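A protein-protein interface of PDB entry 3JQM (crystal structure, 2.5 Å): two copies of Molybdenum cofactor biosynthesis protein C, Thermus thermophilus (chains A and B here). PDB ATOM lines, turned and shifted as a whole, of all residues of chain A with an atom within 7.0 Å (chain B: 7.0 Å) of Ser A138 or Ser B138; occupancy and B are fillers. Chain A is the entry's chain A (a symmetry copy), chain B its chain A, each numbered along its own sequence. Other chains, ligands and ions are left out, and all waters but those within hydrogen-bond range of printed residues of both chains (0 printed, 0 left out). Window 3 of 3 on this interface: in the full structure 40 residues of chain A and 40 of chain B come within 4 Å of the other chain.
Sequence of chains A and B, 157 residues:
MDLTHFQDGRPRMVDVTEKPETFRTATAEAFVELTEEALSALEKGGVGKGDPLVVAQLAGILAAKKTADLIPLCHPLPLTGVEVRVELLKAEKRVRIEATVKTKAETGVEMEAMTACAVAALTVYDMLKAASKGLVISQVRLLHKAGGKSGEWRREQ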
ATOM      1  N   ALA A  30     -21.034  -9.278 -18.619  1.00  0.00           N
ATOM      2  CA  ALA A  30     -21.488  -8.788 -19.903  1.00  0.00           C
ATOM      3  C   ALA A  30     -22.488  -7.684 -19.662  1.00  0.00           C
ATOM      4  O   ALA A  30     -23.254  -7.739 -18.692  1.00  0.00           O
ATOM      5  CB  ALA A  30     -22.149  -9.902 -20.679  1.00  0.00           C
ATOM      6  N   PHE A  31     -22.487  -6.694 -20.554  1.00  0.00           N
ATOM      7  CA  PHE A  31     -23.403  -5.568 -20.457  1.00  0.00           C
ATOM      8  C   PHE A  31     -24.266  -5.417 -21.700  1.00  0.00           C
ATOM      9  O   PHE A  31     -23.839  -5.727 -22.808  1.00  0.00           O
ATOM     10  CB  PHE A  31     -22.639  -4.260 -20.226  1.00  0.00           C
ATOM     11  CG  PHE A  31     -22.043  -4.138 -18.857  1.00  0.00           C
ATOM     12  CD1 PHE A  31     -20.674  -4.332 -18.658  1.00  0.00           C
ATOM     13  CD2 PHE A  31     -22.848  -3.837 -17.758  1.00  0.00           C
ATOM     14  CE1 PHE A  31     -20.113  -4.227 -17.382  1.00  0.00           C
ATOM     15  CE2 PHE A  31     -22.300  -3.730 -16.481  1.00  0.00           C
ATOM     16  CZ  PHE A  31     -20.928  -3.924 -16.292  1.00  0.00           C
ATOM     17  N   VAL A  32     -25.484  -4.931 -21.497  1.00  0.00           N
ATOM     18  CA  VAL A  32     -26.433  -4.696 -22.578  1.00  0.00           C
ATOM     19  C   VAL A  32     -26.998  -3.283 -22.438  1.00  0.00           C
ATOM     20  O   VAL A  32     -27.790  -3.018 -21.527  1.00  0.00           O
ATOM     21  CB  VAL A  32     -27.597  -5.706 -22.527  1.00  0.00           C
ATOM     22  CG1 VAL A  32     -28.619  -5.405 -23.630  1.00  0.00           C
ATOM     23  CG2 VAL A  32     -27.053  -7.110 -22.674  1.00  0.00           C
ATOM     24  N   GLU A  33     -26.580  -2.390 -23.337  1.00  0.00           N
ATOM     25  CA  GLU A  33     -27.035  -1.004 -23.342  1.00  0.00           C
ATOM     26  C   GLU A  33     -28.494  -0.953 -23.757  1.00  0.00           C
ATOM     27  O   GLU A  33     -28.874  -1.528 -24.771  1.00  0.00           O
ATOM     28  CB  GLU A  33     -26.207  -0.169 -24.323  1.00  0.00           C
ATOM     29  CG  GLU A  33     -24.703  -0.309 -24.163  1.00  0.00           C
ATOM     30  CD  GLU A  33     -24.258  -0.116 -22.730  1.00  0.00           C
ATOM     31  OE1 GLU A  33     -24.848   0.744 -22.042  1.00  0.00           O
ATOM     32  OE2 GLU A  33     -23.312  -0.807 -22.293  1.00  0.00           O
ATOM     33  N   ARG A  94     -28.712  -0.122 -18.337  1.00  0.00           N
ATOM     34  CA  ARG A  94     -27.930  -1.265 -18.737  1.00  0.00           C
ATOM     35  C   ARG A  94     -28.333  -2.494 -17.976  1.00  0.00           C
ATOM     36  O   ARG A  94     -28.816  -2.419 -16.847  1.00  0.00           O
ATOM     37  CB  ARG A  94     -26.444  -1.010 -18.486  1.00  0.00           C
ATOM     38  CG  ARG A  94     -25.722  -0.386 -19.668  1.00  0.00           C
ATOM     39  CD  ARG A  94     -24.463   0.395 -19.269  1.00  0.00           C
ATOM     40  NE  ARG A  94     -23.344  -0.445 -18.854  1.00  0.00           N
ATOM     41  CZ  ARG A  94     -22.110   0.014 -18.687  1.00  0.00           C
ATOM     42  NH1 ARG A  94     -21.857   1.298 -18.902  1.00  0.00           N
ATOM     43  NH2 ARG A  94     -21.127  -0.801 -18.313  1.00  0.00           N
ATOM     44  N   VAL A  95     -28.150  -3.635 -18.623  1.00  0.00           N
ATOM     45  CA  VAL A  95     -28.426  -4.911 -17.999  1.00  0.00           C
ATOM     46  C   VAL A  95     -27.013  -5.413 -17.774  1.00  0.00           C
ATOM     47  O   VAL A  95     -26.145  -5.213 -18.618  1.00  0.00           O
ATOM     48  CB  VAL A  95     -29.171  -5.873 -18.951  1.00  0.00           C
ATOM     49  CG1 VAL A  95     -29.168  -7.280 -18.377  1.00  0.00           C
ATOM     50  CG2 VAL A  95     -30.590  -5.402 -19.153  1.00  0.00           C
ATOM     51  N   ALA A 121     -26.577 -12.442 -22.704  1.00  0.00           N
ATOM     52  CA  ALA A 121     -26.765 -11.125 -23.319  1.00  0.00           C
ATOM     53  C   ALA A 121     -27.568 -11.290 -24.594  1.00  0.00           C
ATOM     54  O   ALA A 121     -28.578 -10.600 -24.789  1.00  0.00           O
ATOM     55  CB  ALA A 121     -25.432 -10.497 -23.638  1.00  0.00           C
ATOM     56  N   VAL A 136     -27.439  -2.749 -27.749  1.00  0.00           N
ATOM     57  CA  VAL A 136     -26.093  -3.273 -27.906  1.00  0.00           C
ATOM     58  C   VAL A 136     -25.553  -4.094 -26.741  1.00  0.00           C
ATOM     59  O   VAL A 136     -25.883  -3.846 -25.571  1.00  0.00           O
ATOM     60  CB  VAL A 136     -25.150  -2.078 -28.159  1.00  0.00           C
ATOM     61  CG1 VAL A 136     -23.745  -2.552 -28.384  1.00  0.00           C
ATOM     62  CG2 VAL A 136     -25.623  -1.302 -29.360  1.00  0.00           C
ATOM     63  N   ILE A 137     -24.745  -5.099 -27.086  1.00  0.00           N
ATOM     64  CA  ILE A 137     -24.074  -5.945 -26.101  1.00  0.00           C
ATOM     65  C   ILE A 137     -22.711  -5.265 -26.101  1.00  0.00           C
ATOM     66  O   ILE A 137     -21.932  -5.436 -27.037  1.00  0.00           O
ATOM     67  CB  ILE A 137     -23.947  -7.397 -26.582  1.00  0.00           C
ATOM     68  CG1 ILE A 137     -25.338  -7.971 -26.876  1.00  0.00           C
ATOM     69  CG2 ILE A 137     -23.244  -8.232 -25.514  1.00  0.00           C
ATOM     70  CD1 ILE A 137     -25.344  -9.392 -27.430  1.00  0.00           C
ATOM     71  N   SER A 138     -22.435  -4.480 -25.059  1.00  0.00           N
ATOM     72  CA  SER A 138     -21.204  -3.696 -24.987  1.00  0.00           C
ATOM     73  C   SER A 138     -19.912  -4.217 -24.369  1.00  0.00           C
ATOM     74  O   SER A 138     -18.830  -3.861 -24.826  1.00  0.00           O
ATOM     75  CB  SER A 138     -21.490  -2.373 -24.272  1.00  0.00           C
ATOM     76  OG  SER A 138     -21.746  -2.569 -22.893  1.00  0.00           O
ATOM     77  N   GLN A 139     -19.989  -5.039 -23.337  1.00  0.00           N
ATOM     78  CA  GLN A 139     -18.745  -5.479 -22.733  1.00  0.00           C
ATOM     79  C   GLN A 139     -18.821  -6.876 -22.184  1.00  0.00           C
ATOM     80  O   GLN A 139     -19.537  -7.133 -21.220  1.00  0.00           O
ATOM     81  CB  GLN A 139     -18.262  -4.563 -21.608  1.00  0.00           C
ATOM     82  CG  GLN A 139     -17.942  -3.132 -22.005  1.00  0.00           C
ATOM     83  CD  GLN A 139     -16.453  -2.839 -21.982  1.00  0.00           C
ATOM     84  OE1 GLN A 139     -15.772  -3.080 -20.980  1.00  0.00           O
ATOM     85  NE2 GLN A 139     -15.938  -2.311 -23.087  1.00  0.00           N
ATOM     86  N   VAL A 140     -18.083  -7.780 -22.805  1.00  0.00           N
ATOM     87  CA  VAL A 140     -18.013  -9.149 -22.333  1.00  0.00           C
ATOM     88  C   VAL A 140     -16.532  -9.298 -22.023  1.00  0.00           C
ATOM     89  O   VAL A 140     -15.700  -9.274 -22.921  1.00  0.00           O
ATOM     90  CB  VAL A 140     -18.463 -10.144 -23.409  1.00  0.00           C
ATOM     91  CG1 VAL A 140     -18.331 -11.561 -22.896  1.00  0.00           C
ATOM     92  CG2 VAL A 140     -19.902  -9.860 -23.780  1.00  0.00           C
ATOM     93  N   ALA B  30     -19.243  -7.490 -34.599  1.00  0.00           N
ATOM     94  CA  ALA B  30     -18.697  -7.658 -33.268  1.00  0.00           C
ATOM     95  C   ALA B  30     -17.259  -7.203 -33.286  1.00  0.00           C
ATOM     96  O   ALA B  30     -16.560  -7.387 -34.290  1.00  0.00           O
ATOM     97  CB  ALA B  30     -18.760  -9.109 -32.860  1.00  0.00           C
ATOM     98  N   PHE B  31     -16.818  -6.625 -32.168  1.00  0.00           N
ATOM     99  CA  PHE B  31     -15.450  -6.148 -32.035  1.00  0.00           C
ATOM    100  C   PHE B  31     -14.725  -6.790 -30.863  1.00  0.00           C
ATOM    101  O   PHE B  31     -15.331  -7.115 -29.846  1.00  0.00           O
ATOM    102  CB  PHE B  31     -15.416  -4.626 -31.861  1.00  0.00           C
ATOM    103  CG  PHE B  31     -15.765  -3.864 -33.103  1.00  0.00           C
ATOM    104  CD1 PHE B  31     -17.020  -3.269 -33.244  1.00  0.00           C
ATOM    105  CD2 PHE B  31     -14.839  -3.743 -34.141  1.00  0.00           C
ATOM    106  CE1 PHE B  31     -17.352  -2.563 -34.404  1.00  0.00           C
ATOM    107  CE2 PHE B  31     -15.159  -3.042 -35.303  1.00  0.00           C
ATOM    108  CZ  PHE B  31     -16.420  -2.449 -35.434  1.00  0.00           C
ATOM    109  N   VAL B  32     -13.419  -6.964 -31.021  1.00  0.00           N
ATOM    110  CA  VAL B  32     -12.566  -7.540 -29.989  1.00  0.00           C
ATOM    111  C   VAL B  32     -11.348  -6.637 -29.797  1.00  0.00           C
ATOM    112  O   VAL B  32     -10.469  -6.588 -30.663  1.00  0.00           O
ATOM    113  CB  VAL B  32     -12.083  -8.949 -30.387  1.00  0.00           C
ATOM    114  CG1 VAL B  32     -11.137  -9.514 -29.323  1.00  0.00           C
ATOM    115  CG2 VAL B  32     -13.280  -9.858 -30.572  1.00  0.00           C
ATOM    116  N   GLU B  33     -11.315  -5.926 -28.668  1.00  0.00           N
ATOM    117  CA  GLU B  33     -10.216  -5.026 -28.335  1.00  0.00           C
ATOM    118  C   GLU B  33      -8.973  -5.840 -28.029  1.00  0.00           C
ATOM    119  O   GLU B  33      -9.017  -6.770 -27.231  1.00  0.00           O
ATOM    120  CB  GLU B  33     -10.569  -4.175 -27.113  1.00  0.00           C
ATOM    121  CG  GLU B  33     -11.916  -3.477 -27.192  1.00  0.00           C
ATOM    122  CD  GLU B  33     -12.093  -2.718 -28.489  1.00  0.00           C
ATOM    123  OE1 GLU B  33     -11.097  -2.137 -28.970  1.00  0.00           O
ATOM    124  OE2 GLU B  33     -13.223  -2.685 -29.020  1.00  0.00           O
ATOM    125  N   ARG B  94      -7.961  -3.859 -33.046  1.00  0.00           N
ATOM    126  CA  ARG B  94      -9.247  -4.498 -32.902  1.00  0.00           C
ATOM    127  C   ARG B  94      -9.475  -5.511 -33.984  1.00  0.00           C
ATOM    128  O   ARG B  94      -8.940  -5.402 -35.087  1.00  0.00           O
ATOM    129  CB  ARG B  94     -10.369  -3.462 -32.967  1.00  0.00           C
ATOM    130  CG  ARG B  94     -10.754  -2.890 -31.614  1.00  0.00           C
ATOM    131  CD  ARG B  94     -11.401  -1.501 -31.702  1.00  0.00           C
ATOM    132  NE  ARG B  94     -12.759  -1.508 -32.238  1.00  0.00           N
ATOM    133  CZ  ARG B  94     -13.568  -0.456 -32.189  1.00  0.00           C
ATOM    134  NH1 ARG B  94     -13.141   0.668 -31.628  1.00  0.00           N
ATOM    135  NH2 ARG B  94     -14.797  -0.523 -32.689  1.00  0.00           N
ATOM    136  N   VAL B  95     -10.264  -6.519 -33.646  1.00  0.00           N
ATOM    137  CA  VAL B  95     -10.636  -7.542 -34.600  1.00  0.00           C
ATOM    138  C   VAL B  95     -12.085  -7.170 -34.843  1.00  0.00           C
ATOM    139  O   VAL B  95     -12.787  -6.782 -33.915  1.00  0.00           O
ATOM    140  CB  VAL B  95     -10.561  -8.959 -33.989  1.00  0.00           C
ATOM    141  CG1 VAL B  95     -11.241  -9.960 -34.907  1.00  0.00           C
ATOM    142  CG2 VAL B  95      -9.120  -9.354 -33.776  1.00  0.00           C
ATOM    143  N   ALA B 121     -16.421 -13.985 -31.898  1.00  0.00           N
ATOM    144  CA  ALA B 121     -15.631 -13.164 -30.978  1.00  0.00           C
ATOM    145  C   ALA B 121     -15.121 -14.043 -29.852  1.00  0.00           C
ATOM    146  O   ALA B 121     -13.917 -14.046 -29.558  1.00  0.00           O
ATOM    147  CB  ALA B 121     -16.473 -12.050 -30.409  1.00  0.00           C
ATOM    148  N   VAL B 136     -11.089  -7.810 -24.578  1.00  0.00           N
ATOM    149  CA  VAL B 136     -12.519  -7.591 -24.464  1.00  0.00           C
ATOM    150  C   VAL B 136     -13.318  -7.682 -25.761  1.00  0.00           C
ATOM    151  O   VAL B 136     -12.822  -7.343 -26.846  1.00  0.00           O
ATOM    152  CB  VAL B 136     -12.734  -6.196 -23.840  1.00  0.00           C
ATOM    153  CG1 VAL B 136     -14.195  -5.923 -23.644  1.00  0.00           C
ATOM    154  CG2 VAL B 136     -12.019  -6.116 -22.516  1.00  0.00           C
ATOM    155  N   ILE B 137     -14.549  -8.181 -25.631  1.00  0.00           N
ATOM    156  CA  ILE B 137     -15.483  -8.272 -26.750  1.00  0.00           C
ATOM    157  C   ILE B 137     -16.303  -7.018 -26.473  1.00  0.00           C
ATOM    158  O   ILE B 137     -17.124  -7.003 -25.559  1.00  0.00           O
ATOM    159  CB  ILE B 137     -16.371  -9.521 -26.656  1.00  0.00           C
ATOM    160  CG1 ILE B 137     -15.497 -10.779 -26.626  1.00  0.00           C
ATOM    161  CG2 ILE B 137     -17.323  -9.565 -27.851  1.00  0.00           C
ATOM    162  CD1 ILE B 137     -16.260 -12.090 -26.464  1.00  0.00           C
ATOM    163  N   SER B 138     -16.060  -5.962 -27.251  1.00  0.00           N
ATOM    164  CA  SER B 138     -16.706  -4.671 -27.025  1.00  0.00           C
ATOM    165  C   SER B 138     -18.032  -4.275 -27.661  1.00  0.00           C
ATOM    166  O   SER B 138     -18.810  -3.548 -27.049  1.00  0.00           O
ATOM    167  CB  SER B 138     -15.731  -3.548 -27.389  1.00  0.00           C
ATOM    168  OG  SER B 138     -15.511  -3.480 -28.787  1.00  0.00           O
ATOM    169  N   GLN B 139     -18.313  -4.717 -28.875  1.00  0.00           N
ATOM    170  CA  GLN B 139     -19.559  -4.282 -29.479  1.00  0.00           C
ATOM    171  C   GLN B 139     -20.168  -5.321 -30.378  1.00  0.00           C
ATOM    172  O   GLN B 139     -19.617  -5.647 -31.425  1.00  0.00           O
ATOM    173  CB  GLN B 139     -19.419  -2.992 -30.288  1.00  0.00           C
ATOM    174  CG  GLN B 139     -18.989  -1.761 -29.509  1.00  0.00           C
ATOM    175  CD  GLN B 139     -20.112  -0.752 -29.345  1.00  0.00           C
ATOM    176  OE1 GLN B 139     -20.744  -0.339 -30.323  1.00  0.00           O
ATOM    177  NE2 GLN B 139     -20.362  -0.344 -28.106  1.00  0.00           N
ATOM    178  N   VAL B 140     -21.309  -5.845 -29.962  1.00  0.00           N
ATOM    179  CA  VAL B 140     -22.035  -6.805 -30.768  1.00  0.00           C
ATOM    180  C   VAL B 140     -23.356  -6.089 -30.996  1.00  0.00           C
ATOM    181  O   VAL B 140     -24.121  -5.877 -30.065  1.00  0.00           O
ATOM    182  CB  VAL B 140     -22.238  -8.131 -30.024  1.00  0.00           C
ATOM    183  CG1 VAL B 140     -23.039  -9.090 -30.878  1.00  0.00           C
ATOM    184  CG2 VAL B 140     -20.888  -8.733 -29.699  1.00  0.00           C
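Val A136 touches Val B140 (CG1 to O, 3.7 Å).
Ser B138 touches Ile A137 (O to O, 3.6 Å).
Ile A137 touches Gln B139 (O to CA, 3.6 Å).
Ser A138 touches Ile B137 (O to O, 3.6 Å).
Gln A139 touches Ile B137.
Val B136 touches Val A140 (CG1 to O, 3.7 Å).
Printed residues of chain B that touch a printed residue of chain A: Val B136, Ile B137, Ser B138, Gln B139 and Val B140.
Hydrophobic or aromatic side chains of chain A that line the printed part of chain B: Val A136, Ile A137 and Val A140.
Among the printed residues, 9 pairs touch across the chains.
The backbone carbonyl oxygen (O) of Phe B31 lies within hydrogen-bond range of the backbone NH (N) of Ser B138 (2.9 Å).
The backbone NH (N) of Glu B33 sits at hydrogen-bond distance from the backbone carbonyl oxygen (O) of Val B136 (2.8 Å).
O of Phe A31 sits at hydrogen-bond distance from N of Ser A138 (2.9 Å).
The backbone NH (N) of Phe A31 sits at hydrogen-bond distance from the backbone carbonyl oxygen (O) of Gln A139.
The backbone carbonyl oxygen of Val A136 lies within hydrogen-bond range of the backbone NH of Glu A33, at 2.8 Å.
The side-chain carboxylate (OE2) of Glu A33 sits at hydrogen-bond distance from the side-chain hydroxyl (OG) of Ser A138 (2.4 Å).
Val A136 touches Val B140, and with the chains exchanged Val A140 touches Val B136.
Ile A137 touches Ser B138, and with the chains exchanged Ser A138 touches Ile B137.
Ile A137 touches Gln B139, and with the chains exchanged Gln A139 touches Ile B137.
Ile A137 touches Val B140, and with the chains exchanged Val A140 touches Ile B137.
12 positions are printed for both chains.
Of the 9 pairs that touch across the chains among the printed residues, 9 have their exchanged pair printed and touching as well.
The backbone carbonyl oxygen (O) of Ile B137 lies within hydrogen-bond range of the backbone NH (N) of Val A140, 3.0 Å away.
The backbone NH (N) of Val B140 is in hydrogen-bond range of the backbone carbonyl oxygen (O) of Ile A137 (3.0 Å).
The backbone carbonyl oxygen of Ser A138 sits close to the backbone carbonyl oxygen of Ser B138.
Of chain B, only Ile B137 and Ser B138 come within 4 Å of Ser A138.
Ser B138 touches two residues of chain A.
Printed residues of chain A within 4 Å of Val B140: Val A136 (3.7 Å) and Ile A137 (3.0 Å).
Of the printed residues of chain B, Val A140 touches Val B136 (3.7 Å) and Ile B137 (3.0 Å).
Of the printed residues of chain B, Ile A137 touches Ser B138, Gln B139 and Val B140.
The nearest residue of chain B that does not touch Ser A138 is Gln B139 (4.2 Å).
The nearest residue of chain A that does not touch Ser B138 is Gln A139 (4.2 Å).
The nearest printed residue of chain B that does not touch Ile A137 is Ile B137 (5.3 Å).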
